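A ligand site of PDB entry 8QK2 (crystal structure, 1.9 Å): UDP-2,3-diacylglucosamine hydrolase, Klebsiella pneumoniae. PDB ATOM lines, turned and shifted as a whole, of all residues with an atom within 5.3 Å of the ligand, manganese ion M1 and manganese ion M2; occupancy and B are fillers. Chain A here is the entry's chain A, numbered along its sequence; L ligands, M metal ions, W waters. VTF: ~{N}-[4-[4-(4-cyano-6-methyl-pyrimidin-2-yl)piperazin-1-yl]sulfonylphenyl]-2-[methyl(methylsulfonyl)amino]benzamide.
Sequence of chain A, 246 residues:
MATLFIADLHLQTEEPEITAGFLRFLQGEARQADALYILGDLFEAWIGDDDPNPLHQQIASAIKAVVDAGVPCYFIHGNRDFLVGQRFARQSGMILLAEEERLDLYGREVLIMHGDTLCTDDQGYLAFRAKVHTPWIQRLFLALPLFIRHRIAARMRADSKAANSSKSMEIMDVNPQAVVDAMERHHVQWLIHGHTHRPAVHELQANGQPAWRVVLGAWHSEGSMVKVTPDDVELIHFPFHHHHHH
Of the 29 residues printed, 4 come within 4 Å of manganese ion M2.
OD1 of Asp 8 is bound to manganese ion M2 (2.1 Å).
Water W1 binds manganese ion M2 (2.1 Å).
NE2 of His 10 binds manganese ion M2, at 2.2 Å.
NE2 of His 197 is bound to manganese ion M2 (2.2 Å).
OD2 of Asp 41 is bound to manganese ion M2 (2.2 Å).
Manganese ion M2 has five donor atoms within binding distance.
Manganese ion M1 is bound by OD2 of Asp 41, OD1 of Asn 79, water W1, ND1 of His 195 and NE2 of His 114.
The guanidinium group (NH1) of Arg 80 lies within hydrogen-bond range of an oxygen (O36) of the ligand (2.9 Å).
An oxygen (O15) of the ligand is in hydrogen-bond range of the backbone NH of Trp 46 (3.0 Å).
O24 of the ligand sits at hydrogen-bond distance from ND2 of Asn 79 (3.1 Å).
The side-chain carboxylate of Asp 8 sits at hydrogen-bond distance from the backbone NH of His 195, 2.8 Å away.
The side-chain amide nitrogen (NE2) of Gln 138 sits at hydrogen-bond distance from the backbone carbonyl oxygen (O) of Val 132, 2.6 Å away.
ND1 of His 10 is in hydrogen-bond range of OE1 of Glu 44.
The side-chain carboxylate (OD1) of Asp 41 sits at hydrogen-bond distance from the backbone NH (N) of Arg 80, at 3.1 Å.
The guanidinium group (NH2) of Arg 80 lies within salt-bridge range of the side-chain carboxylate (OE2) of Glu 44 (3.5 Å).
The side-chain carboxylate (OD1) of Asp 122 is in hydrogen-bond range of the backbone NH (N) of Tyr 125 (3.0 Å).
The side-chain hydroxyl of Tyr 125 sits at hydrogen-bond distance from the side-chain carboxylate of Asp 116.
Within 4 Å of manganese ion M1: Asp 8, Asp 41, Asn 79, His 114 and His 195.
The nearest printed residue that does not touch manganese ion M1 is His 197 (5.0 Å).
Merely in contact with the ligand: Ala 45 (3.2 Å), Met 156 (3.3 Å), Phe 141 (3.4 Å), Phe 128 (3.5 Å), Leu 83 (3.7 Å), Tyr 125 (3.7 Å), Phe 82 (3.7 Å), Ile 137 (3.8 Å), Gln 138 (3.9 Å), Ile 152 (3.9 Å) and Ala 153 (3.98 Å).
Hydrophobic or aromatic side chains that line the ligand: Ala 45, Phe 82, Leu 83, Tyr 125, Phe 128, Phe 141, Ile 152, Ala 153 and Met 156.
14 residues have an atom within 4 Å of the ligand: Ala 45, Trp 46, Asn 79, Arg 80, Phe 82, Leu 83, Tyr 125, Phe 128, Ile 137, Gln 138, Phe 141, Ile 152, Ala 153 and Met 156.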
ATOM      1  N   ASP A   8      17.526  -7.405  29.190  1.00  0.00           N
ATOM      2  CA  ASP A   8      16.644  -8.496  29.556  1.00  0.00           C
ATOM      3  C   ASP A   8      16.582  -8.698  31.079  1.00  0.00           C
ATOM      4  O   ASP A   8      16.501  -9.838  31.547  1.00  0.00           O
ATOM      5  CB  ASP A   8      17.019  -9.791  28.819  1.00  0.00           C
ATOM      6  CG  ASP A   8      16.949  -9.640  27.317  1.00  0.00           C
ATOM      7  OD1 ASP A   8      15.843  -9.465  26.797  1.00  0.00           O
ATOM      8  OD2 ASP A   8      18.007  -9.654  26.661  1.00  0.00           O
ATOM      9  N   HIS A  10      13.873  -7.614  32.695  1.00  0.00           N
ATOM     10  CA  HIS A  10      12.459  -7.930  32.875  1.00  0.00           C
ATOM     11  C   HIS A  10      11.968  -7.536  34.273  1.00  0.00           C
ATOM     12  O   HIS A  10      11.284  -8.309  34.928  1.00  0.00           O
ATOM     13  CB  HIS A  10      12.200  -9.398  32.515  1.00  0.00           C
ATOM     14  CG  HIS A  10      12.391  -9.669  31.062  1.00  0.00           C
ATOM     15  ND1 HIS A  10      11.305  -9.709  30.208  1.00  0.00           N
ATOM     16  CD2 HIS A  10      13.464  -9.872  30.306  1.00  0.00           C
ATOM     17  CE1 HIS A  10      11.734  -9.929  28.973  1.00  0.00           C
ATOM     18  NE2 HIS A  10      13.039 -10.032  29.015  1.00  0.00           N
ATOM     19  N   ASP A  41      14.316  -4.495  27.176  1.00  0.00           N
ATOM     20  CA  ASP A  41      13.662  -5.358  28.150  1.00  0.00           C
ATOM     21  C   ASP A  41      14.250  -5.098  29.536  1.00  0.00           C
ATOM     22  O   ASP A  41      14.506  -6.024  30.300  1.00  0.00           O
ATOM     23  CB  ASP A  41      13.786  -6.840  27.738  1.00  0.00           C
ATOM     24  CG  ASP A  41      12.948  -7.248  26.530  1.00  0.00           C
ATOM     25  OD1 ASP A  41      12.202  -6.378  26.003  1.00  0.00           O
ATOM     26  OD2 ASP A  41      13.086  -8.452  26.123  1.00  0.00           O
ATOM     27  N   GLU A  44       9.553  -5.677  32.346  1.00  0.00           N
ATOM     28  CA  GLU A  44       8.735  -6.776  31.865  1.00  0.00           C
ATOM     29  C   GLU A  44       7.565  -6.266  31.028  1.00  0.00           C
ATOM     30  O   GLU A  44       7.053  -7.005  30.178  1.00  0.00           O
ATOM     31  CB  GLU A  44       8.196  -7.587  33.051  1.00  0.00           C
ATOM     32  CG  GLU A  44       7.221  -8.698  32.682  1.00  0.00           C
ATOM     33  CD  GLU A  44       7.723  -9.746  31.708  1.00  0.00           C
ATOM     34  OE1 GLU A  44       8.958  -9.841  31.484  1.00  0.00           O
ATOM     35  OE2 GLU A  44       6.873 -10.467  31.145  1.00  0.00           O
ATOM     36  N   ALA A  45       7.127  -5.036  31.314  1.00  0.00           N
ATOM     37  CA  ALA A  45       6.006  -4.400  30.638  1.00  0.00           C
ATOM     38  C   ALA A  45       6.126  -2.884  30.765  1.00  0.00           C
ATOM     39  O   ALA A  45       6.700  -2.362  31.721  1.00  0.00           O
ATOM     40  CB  ALA A  45       4.689  -4.860  31.224  1.00  0.00           C
ATOM     41  N   TRP A  46       5.508  -2.186  29.802  1.00  0.00           N
ATOM     42  CA  TRP A  46       5.392  -0.751  29.902  1.00  0.00           C
ATOM     43  C   TRP A  46       4.144  -0.308  29.132  1.00  0.00           C
ATOM     44  O   TRP A  46       3.936  -0.733  28.003  1.00  0.00           O
ATOM     45  CB  TRP A  46       6.664  -0.088  29.394  1.00  0.00           C
ATOM     46  CG  TRP A  46       6.878   1.308  29.871  1.00  0.00           C
ATOM     47  CD1 TRP A  46       6.493   2.461  29.238  1.00  0.00           C
ATOM     48  CD2 TRP A  46       7.590   1.707  31.045  1.00  0.00           C
ATOM     49  NE1 TRP A  46       6.910   3.552  29.955  1.00  0.00           N
ATOM     50  CE2 TRP A  46       7.583   3.118  31.072  1.00  0.00           C
ATOM     51  CE3 TRP A  46       8.232   1.017  32.087  1.00  0.00           C
ATOM     52  CZ2 TRP A  46       8.201   3.849  32.090  1.00  0.00           C
ATOM     53  CZ3 TRP A  46       8.856   1.745  33.084  1.00  0.00           C
ATOM     54  CH2 TRP A  46       8.830   3.144  33.082  1.00  0.00           C
ATOM     55  N   ILE A  47       3.293   0.478  29.802  1.00  0.00           N
ATOM     56  CA  ILE A  47       2.050   0.967  29.209  1.00  0.00           C
ATOM     57  C   ILE A  47       2.060   2.482  29.182  1.00  0.00           C
ATOM     58  O   ILE A  47       1.051   3.089  28.836  1.00  0.00           O
ATOM     59  CB  ILE A  47       0.825   0.417  29.954  1.00  0.00           C
ATOM     60  CG1 ILE A  47       0.769   0.924  31.403  1.00  0.00           C
ATOM     61  CG2 ILE A  47       0.797  -1.097  29.860  1.00  0.00           C
ATOM     62  CD1 ILE A  47      -0.538   0.641  32.106  1.00  0.00           C
ATOM     63  N   GLY A  78      13.390  -2.688  24.054  1.00  0.00           N
ATOM     64  CA  GLY A  78      13.064  -4.074  23.742  1.00  0.00           C
ATOM     65  C   GLY A  78      11.641  -4.218  23.195  1.00  0.00           C
ATOM     66  O   GLY A  78      10.964  -3.235  22.942  1.00  0.00           O
ATOM     67  N   ASN A  79      11.210  -5.464  23.000  1.00  0.00           N
ATOM     68  CA  ASN A  79       9.843  -5.747  22.609  1.00  0.00           C
ATOM     69  C   ASN A  79       8.890  -5.480  23.770  1.00  0.00           C
ATOM     70  O   ASN A  79       7.693  -5.233  23.558  1.00  0.00           O
ATOM     71  CB  ASN A  79       9.638  -7.178  22.097  1.00  0.00           C
ATOM     72  CG  ASN A  79      10.195  -8.210  23.044  1.00  0.00           C
ATOM     73  OD1 ASN A  79      11.367  -8.113  23.387  1.00  0.00           O
ATOM     74  ND2 ASN A  79       9.400  -9.167  23.487  1.00  0.00           N
ATOM     75  N   ARG A  80       9.397  -5.594  25.004  1.00  0.00           N
ATOM     76  CA  ARG A  80       8.540  -5.512  26.173  1.00  0.00           C
ATOM     77  C   ARG A  80       8.303  -4.045  26.537  1.00  0.00           C
ATOM     78  O   ARG A  80       7.216  -3.728  27.011  1.00  0.00           O
ATOM     79  CB  ARG A  80       9.146  -6.247  27.375  1.00  0.00           C
ATOM     80  CG  ARG A  80       9.328  -7.751  27.193  1.00  0.00           C
ATOM     81  CD  ARG A  80       8.077  -8.523  26.836  1.00  0.00           C
ATOM     82  NE  ARG A  80       7.019  -8.456  27.840  1.00  0.00           N
ATOM     83  CZ  ARG A  80       5.838  -9.060  27.737  1.00  0.00           C
ATOM     84  NH1 ARG A  80       5.565  -9.854  26.706  1.00  0.00           N
ATOM     85  NH2 ARG A  80       4.934  -8.895  28.679  1.00  0.00           N
ATOM     86  N   PHE A  82       8.896  -1.015  24.670  1.00  0.00           N
ATOM     87  CA  PHE A  82       8.978  -0.093  23.554  1.00  0.00           C
ATOM     88  C   PHE A  82       8.276   1.253  23.808  1.00  0.00           C
ATOM     89  O   PHE A  82       8.546   2.200  23.077  1.00  0.00           O
ATOM     90  CB  PHE A  82       8.412  -0.750  22.292  1.00  0.00           C
ATOM     91  CG  PHE A  82       6.975  -1.162  22.384  1.00  0.00           C
ATOM     92  CD1 PHE A  82       5.954  -0.278  22.078  1.00  0.00           C
ATOM     93  CD2 PHE A  82       6.643  -2.461  22.753  1.00  0.00           C
ATOM     94  CE1 PHE A  82       4.630  -0.683  22.133  1.00  0.00           C
ATOM     95  CE2 PHE A  82       5.322  -2.857  22.823  1.00  0.00           C
ATOM     96  CZ  PHE A  82       4.322  -1.960  22.532  1.00  0.00           C
ATOM     97  N   LEU A  83       7.436   1.344  24.844  1.00  0.00           N
ATOM     98  CA  LEU A  83       6.687   2.568  25.129  1.00  0.00           C
ATOM     99  C   LEU A  83       7.440   3.448  26.121  1.00  0.00           C
ATOM    100  O   LEU A  83       6.982   4.532  26.460  1.00  0.00           O
ATOM    101  CB  LEU A  83       5.280   2.215  25.642  1.00  0.00           C
ATOM    102  CG  LEU A  83       4.271   1.734  24.600  1.00  0.00           C
ATOM    103  CD1 LEU A  83       2.882   1.567  25.188  1.00  0.00           C
ATOM    104  CD2 LEU A  83       4.224   2.704  23.408  1.00  0.00           C
ATOM    105  N   HIS A 114      18.584  -4.504  20.441  1.00  0.00           N
ATOM    106  CA  HIS A 114      17.889  -5.455  21.306  1.00  0.00           C
ATOM    107  C   HIS A 114      18.062  -6.888  20.792  1.00  0.00           C
ATOM    108  O   HIS A 114      18.369  -7.783  21.580  1.00  0.00           O
ATOM    109  CB  HIS A 114      16.408  -5.130  21.500  1.00  0.00           C
ATOM    110  CG  HIS A 114      15.758  -6.017  22.502  1.00  0.00           C
ATOM    111  ND1 HIS A 114      16.219  -6.124  23.805  1.00  0.00           N
ATOM    112  CD2 HIS A 114      14.747  -6.903  22.390  1.00  0.00           C
ATOM    113  CE1 HIS A 114      15.470  -7.010  24.442  1.00  0.00           C
ATOM    114  NE2 HIS A 114      14.561  -7.488  23.604  1.00  0.00           N
ATOM    115  N   ASP A 116      15.562  -8.404  18.698  1.00  0.00           N
ATOM    116  CA  ASP A 116      14.274  -8.883  18.217  1.00  0.00           C
ATOM    117  C   ASP A 116      14.138  -8.692  16.705  1.00  0.00           C
ATOM    118  O   ASP A 116      13.499  -9.524  16.045  1.00  0.00           O
ATOM    119  CB  ASP A 116      13.117  -8.240  18.990  1.00  0.00           C
ATOM    120  CG  ASP A 116      13.029  -6.732  18.824  1.00  0.00           C
ATOM    121  OD1 ASP A 116      14.011  -6.028  19.187  1.00  0.00           O
ATOM    122  OD2 ASP A 116      11.985  -6.256  18.304  1.00  0.00           O
ATOM    123  N   ASP A 122      10.008 -15.265  12.879  1.00  0.00           N
ATOM    124  CA  ASP A 122       8.774 -15.146  13.655  1.00  0.00           C
ATOM    125  C   ASP A 122       7.883 -14.109  12.988  1.00  0.00           C
ATOM    126  O   ASP A 122       8.014 -12.920  13.274  1.00  0.00           O
ATOM    127  CB  ASP A 122       9.066 -14.846  15.125  1.00  0.00           C
ATOM    128  CG  ASP A 122       7.864 -15.084  16.018  1.00  0.00           C
ATOM    129  OD1 ASP A 122       6.727 -15.102  15.487  1.00  0.00           O
ATOM    130  OD2 ASP A 122       8.068 -15.293  17.222  1.00  0.00           O
ATOM    131  N   GLY A 124       4.525 -13.747  13.153  1.00  0.00           N
ATOM    132  CA  GLY A 124       3.648 -13.248  14.207  1.00  0.00           C
ATOM    133  C   GLY A 124       4.287 -12.104  14.991  1.00  0.00           C
ATOM    134  O   GLY A 124       3.702 -11.032  15.091  1.00  0.00           O
ATOM    135  N   TYR A 125       5.489 -12.322  15.536  1.00  0.00           N
ATOM    136  CA  TYR A 125       6.123 -11.262  16.291  1.00  0.00           C
ATOM    137  C   TYR A 125       6.299 -10.018  15.405  1.00  0.00           C
ATOM    138  O   TYR A 125       5.966  -8.904  15.829  1.00  0.00           O
ATOM    139  CB  TYR A 125       7.477 -11.658  16.884  1.00  0.00           C
ATOM    140  CG  TYR A 125       8.119 -10.454  17.499  1.00  0.00           C
ATOM    141  CD1 TYR A 125       7.507  -9.809  18.555  1.00  0.00           C
ATOM    142  CD2 TYR A 125       9.235  -9.852  16.933  1.00  0.00           C
ATOM    143  CE1 TYR A 125       8.017  -8.631  19.078  1.00  0.00           C
ATOM    144  CE2 TYR A 125       9.765  -8.683  17.451  1.00  0.00           C
ATOM    145  CZ  TYR A 125       9.140  -8.065  18.519  1.00  0.00           C
ATOM    146  OH  TYR A 125       9.627  -6.888  19.035  1.00  0.00           O
ATOM    147  N   PHE A 128       3.289  -7.923  14.776  1.00  0.00           N
ATOM    148  CA  PHE A 128       3.007  -7.211  16.018  1.00  0.00           C
ATOM    149  C   PHE A 128       3.912  -5.984  16.137  1.00  0.00           C
ATOM    150  O   PHE A 128       3.455  -4.875  16.364  1.00  0.00           O
ATOM    151  CB  PHE A 128       3.141  -8.197  17.186  1.00  0.00           C
ATOM    152  CG  PHE A 128       3.075  -7.596  18.572  1.00  0.00           C
ATOM    153  CD1 PHE A 128       1.870  -7.408  19.216  1.00  0.00           C
ATOM    154  CD2 PHE A 128       4.242  -7.268  19.244  1.00  0.00           C
ATOM    155  CE1 PHE A 128       1.823  -6.877  20.503  1.00  0.00           C
ATOM    156  CE2 PHE A 128       4.200  -6.727  20.517  1.00  0.00           C
ATOM    157  CZ  PHE A 128       2.989  -6.536  21.139  1.00  0.00           C
ATOM    158  N   VAL A 132       2.974  -1.911  16.659  1.00  0.00           N
ATOM    159  CA  VAL A 132       3.202  -1.149  17.878  1.00  0.00           C
ATOM    160  C   VAL A 132       4.334  -0.141  17.694  1.00  0.00           C
ATOM    161  O   VAL A 132       4.541   0.698  18.566  1.00  0.00           O
ATOM    162  CB  VAL A 132       3.450  -2.066  19.102  1.00  0.00           C
ATOM    163  CG1 VAL A 132       2.297  -3.033  19.321  1.00  0.00           C
ATOM    164  CG2 VAL A 132       4.766  -2.825  19.022  1.00  0.00           C
ATOM    165  N   ILE A 137      -0.416   4.472  16.215  1.00  0.00           N
ATOM    166  CA  ILE A 137      -0.938   3.382  17.030  1.00  0.00           C
ATOM    167  C   ILE A 137      -0.428   3.522  18.460  1.00  0.00           C
ATOM    168  O   ILE A 137      -1.155   3.228  19.396  1.00  0.00           O
ATOM    169  CB  ILE A 137      -0.614   2.018  16.404  1.00  0.00           C
ATOM    170  CG1 ILE A 137      -1.252   1.889  15.018  1.00  0.00           C
ATOM    171  CG2 ILE A 137      -1.011   0.870  17.323  1.00  0.00           C
ATOM    172  CD1 ILE A 137      -1.151   0.512  14.408  1.00  0.00           C
ATOM    173  N   GLN A 138       0.816   3.997  18.649  1.00  0.00           N
ATOM    174  CA  GLN A 138       1.306   4.225  19.993  1.00  0.00           C
ATOM    175  C   GLN A 138       0.529   5.338  20.693  1.00  0.00           C
ATOM    176  O   GLN A 138       0.225   5.221  21.880  1.00  0.00           O
ATOM    177  CB  GLN A 138       2.795   4.568  19.980  1.00  0.00           C
ATOM    178  CG  GLN A 138       3.675   3.387  19.617  1.00  0.00           C
ATOM    179  CD  GLN A 138       5.136   3.669  19.807  1.00  0.00           C
ATOM    180  OE1 GLN A 138       5.533   4.808  20.055  1.00  0.00           O
ATOM    181  NE2 GLN A 138       5.963   2.635  19.670  1.00  0.00           N
ATOM    182  N   PHE A 141      -2.921   4.380  21.903  1.00  0.00           N
ATOM    183  CA  PHE A 141      -2.907   3.545  23.095  1.00  0.00           C
ATOM    184  C   PHE A 141      -2.630   4.417  24.304  1.00  0.00           C
ATOM    185  O   PHE A 141      -3.296   4.268  25.316  1.00  0.00           O
ATOM    186  CB  PHE A 141      -1.856   2.444  22.990  1.00  0.00           C
ATOM    187  CG  PHE A 141      -1.757   1.559  24.214  1.00  0.00           C
ATOM    188  CD1 PHE A 141      -2.662   0.539  24.423  1.00  0.00           C
ATOM    189  CD2 PHE A 141      -0.776   1.772  25.158  1.00  0.00           C
ATOM    190  CE1 PHE A 141      -2.547  -0.284  25.536  1.00  0.00           C
ATOM    191  CE2 PHE A 141      -0.663   0.961  26.277  1.00  0.00           C
ATOM    192  CZ  PHE A 141      -1.548  -0.067  26.466  1.00  0.00           C
ATOM    193  N   ILE A 152      -6.033  -3.764  28.966  1.00  0.00           N
ATOM    194  CA  ILE A 152      -5.582  -4.220  27.658  1.00  0.00           C
ATOM    195  C   ILE A 152      -4.389  -5.164  27.838  1.00  0.00           C
ATOM    196  O   ILE A 152      -4.394  -6.267  27.291  1.00  0.00           O
ATOM    197  CB  ILE A 152      -5.310  -3.027  26.711  1.00  0.00           C
ATOM    198  CG1 ILE A 152      -6.618  -2.351  26.288  1.00  0.00           C
ATOM    199  CG2 ILE A 152      -4.497  -3.459  25.506  1.00  0.00           C
ATOM    200  CD1 ILE A 152      -6.455  -0.941  25.778  1.00  0.00           C
ATOM    201  N   ALA A 153      -3.415  -4.768  28.657  1.00  0.00           N
ATOM    202  CA  ALA A 153      -2.252  -5.594  28.936  1.00  0.00           C
ATOM    203  C   ALA A 153      -2.650  -6.928  29.577  1.00  0.00           C
ATOM    204  O   ALA A 153      -2.169  -7.986  29.161  1.00  0.00           O
ATOM    205  CB  ALA A 153      -1.298  -4.831  29.823  1.00  0.00           C
ATOM    206  N   MET A 156      -4.167  -9.425  27.292  1.00  0.00           N
ATOM    207  CA  MET A 156      -3.191  -9.972  26.355  1.00  0.00           C
ATOM    208  C   MET A 156      -2.521 -11.204  26.937  1.00  0.00           C
ATOM    209  O   MET A 156      -2.435 -12.233  26.275  1.00  0.00           O
ATOM    210  CB  MET A 156      -2.117  -8.933  26.013  1.00  0.00           C
ATOM    211  CG  MET A 156      -2.532  -8.001  24.894  1.00  0.00           C
ATOM    212  SD  MET A 156      -1.267  -6.773  24.550  1.00  0.00           S
ATOM    213  CE  MET A 156      -2.169  -5.620  23.530  1.00  0.00           C
ATOM    214  N   GLU A 170       8.534 -19.494  25.051  1.00  0.00           N
ATOM    215  CA  GLU A 170       9.805 -19.564  24.263  1.00  0.00           C
ATOM    216  C   GLU A 170       9.923 -18.348  23.359  1.00  0.00           C
ATOM    217  O   GLU A 170       8.931 -17.861  22.814  1.00  0.00           O
ATOM    218  CB  GLU A 170       9.864 -20.848  23.440  1.00  0.00           C
ATOM    219  CG  GLU A 170      10.456 -22.030  24.189  1.00  0.00           C
ATOM    220  CD  GLU A 170      11.003 -23.111  23.273  1.00  0.00           C
ATOM    221  OE1 GLU A 170      10.453 -24.236  23.293  1.00  0.00           O
ATOM    222  OE2 GLU A 170      11.969 -22.830  22.539  1.00  0.00           O
ATOM    223  N   ILE A 171      11.158 -17.857  23.208  1.00  0.00           N
ATOM    224  CA  ILE A 171      11.464 -16.736  22.340  1.00  0.00           C
ATOM    225  C   ILE A 171      12.252 -17.278  21.139  1.00  0.00           C
ATOM    226  O   ILE A 171      13.262 -17.934  21.314  1.00  0.00           O
ATOM    227  CB  ILE A 171      12.225 -15.646  23.137  1.00  0.00           C
ATOM    228  CG1 ILE A 171      11.343 -15.081  24.262  1.00  0.00           C
ATOM    229  CG2 ILE A 171      12.739 -14.549  22.222  1.00  0.00           C
ATOM    230  CD1 ILE A 171      12.040 -14.075  25.147  1.00  0.00           C
ATOM    231  N   HIS A 195      17.571 -10.195  23.934  1.00  0.00           N
ATOM    232  CA  HIS A 195      16.279 -10.649  23.439  1.00  0.00           C
ATOM    233  C   HIS A 195      16.099 -12.178  23.507  1.00  0.00           C
ATOM    234  O   HIS A 195      15.049 -12.641  23.951  1.00  0.00           O
ATOM    235  CB  HIS A 195      15.971 -10.135  22.022  1.00  0.00           C
ATOM    236  CG  HIS A 195      14.621 -10.576  21.580  1.00  0.00           C
ATOM    237  ND1 HIS A 195      13.463 -10.246  22.242  1.00  0.00           N
ATOM    238  CD2 HIS A 195      14.268 -11.390  20.581  1.00  0.00           C
ATOM    239  CE1 HIS A 195      12.439 -10.824  21.624  1.00  0.00           C
ATOM    240  NE2 HIS A 195      12.899 -11.513  20.610  1.00  0.00           N
ATOM    241  N   HIS A 197      17.642 -14.507  25.114  1.00  0.00           N
ATOM    242  CA  HIS A 197      17.867 -15.133  26.419  1.00  0.00           C
ATOM    243  C   HIS A 197      18.764 -16.374  26.304  1.00  0.00           C
ATOM    244  O   HIS A 197      18.634 -17.275  27.113  1.00  0.00           O
ATOM    245  CB  HIS A 197      16.536 -15.471  27.120  1.00  0.00           C
ATOM    246  CG  HIS A 197      15.633 -14.299  27.390  1.00  0.00           C
ATOM    247  ND1 HIS A 197      14.428 -14.407  28.050  1.00  0.00           N
ATOM    248  CD2 HIS A 197      15.793 -12.994  27.112  1.00  0.00           C
ATOM    249  CE1 HIS A 197      13.867 -13.213  28.125  1.00  0.00           C
ATOM    250  NE2 HIS A 197      14.672 -12.333  27.562  1.00  0.00           N
HETATM  251  C5  VTF L   1       0.133  -0.515  21.821  1.00  0.00           C
HETATM  252  C6  VTF L   1      -1.144  -0.871  21.462  1.00  0.00           C
HETATM  253  N7  VTF L   1       0.692  -2.676  24.656  1.00  0.00           N
HETATM  254  C8  VTF L   1       1.734  -1.898  25.272  1.00  0.00           C
HETATM  255  C9  VTF L   1       2.722  -2.898  25.859  1.00  0.00           C
HETATM  256  C10 VTF L   1      -0.139  -3.309  25.640  1.00  0.00           C
HETATM  257  C11 VTF L   1       0.742  -4.385  26.327  1.00  0.00           C
HETATM  258  C1  VTF L   1      -1.805  -1.864  22.186  1.00  0.00           C
HETATM  259  N2  VTF L   1      -1.209  -2.426  23.249  1.00  0.00           N
HETATM  260  C3  VTF L   1       0.005  -2.000  23.648  1.00  0.00           C
HETATM  261  N4  VTF L   1       0.693  -1.105  22.902  1.00  0.00           N
HETATM  262  N12 VTF L   1       2.024  -3.754  26.860  1.00  0.00           N
HETATM  263  S13 VTF L   1       3.071  -4.901  27.475  1.00  0.00           S
HETATM  264  C14 VTF L   1       3.465  -6.111  26.253  1.00  0.00           C
HETATM  265  O15 VTF L   1       4.259  -4.226  27.941  1.00  0.00           O
HETATM  266  O16 VTF L   1       2.410  -5.524  28.552  1.00  0.00           O
HETATM  267  C17 VTF L   1       2.608  -7.148  26.061  1.00  0.00           C
HETATM  268  C18 VTF L   1       2.865  -8.100  25.097  1.00  0.00           C
HETATM  269  C19 VTF L   1       4.017  -8.052  24.319  1.00  0.00           C
HETATM  270  C20 VTF L   1       4.661  -6.016  25.471  1.00  0.00           C
HETATM  271  C21 VTF L   1       4.920  -7.001  24.492  1.00  0.00           C
HETATM  272  N22 VTF L   1       4.157  -9.028  23.321  1.00  0.00           N
HETATM  273  C23 VTF L   1       5.328  -9.331  22.659  1.00  0.00           C
HETATM  274  O24 VTF L   1       6.378  -8.763  22.925  1.00  0.00           O
HETATM  275  C25 VTF L   1       5.272 -10.426  21.600  1.00  0.00           C
HETATM  276  C26 VTF L   1       4.228 -10.427  20.684  1.00  0.00           C
HETATM  277  C27 VTF L   1       4.149 -11.439  19.731  1.00  0.00           C
HETATM  278  C28 VTF L   1       5.074 -12.467  19.720  1.00  0.00           C
HETATM  279  C29 VTF L   1       6.109 -12.484  20.649  1.00  0.00           C
HETATM  280  C30 VTF L   1       6.200 -11.477  21.617  1.00  0.00           C
HETATM  281  N31 VTF L   1       7.317 -11.465  22.557  1.00  0.00           N
HETATM  282  C32 VTF L   1       8.505 -12.140  21.990  1.00  0.00           C
HETATM  283  S33 VTF L   1       6.899 -12.153  23.978  1.00  0.00           S
HETATM  284  C34 VTF L   1       6.787 -13.921  23.784  1.00  0.00           C
HETATM  285  O35 VTF L   1       7.883 -11.822  24.966  1.00  0.00           O
HETATM  286  O36 VTF L   1       5.652 -11.643  24.391  1.00  0.00           O
HETATM  287  C37 VTF L   1       0.915   0.536  21.046  1.00  0.00           C
HETATM  288  C38 VTF L   1      -3.118  -2.248  21.833  1.00  0.00           C
HETATM  289  N39 VTF L   1      -4.167  -2.646  21.662  1.00  0.00           N
HETATM  290 MN    MN M   1      13.102  -9.107  24.103  1.00  0.00          MN
HETATM  291 MN    MN M   2      13.954 -10.307  27.052  1.00  0.00          MN
HETATM  292  O   HOH W   1      13.353 -11.001  25.136  1.00  0.00           O
HETATM  293  O   HOH W   2       2.035 -10.892  23.238  1.00  0.00           O
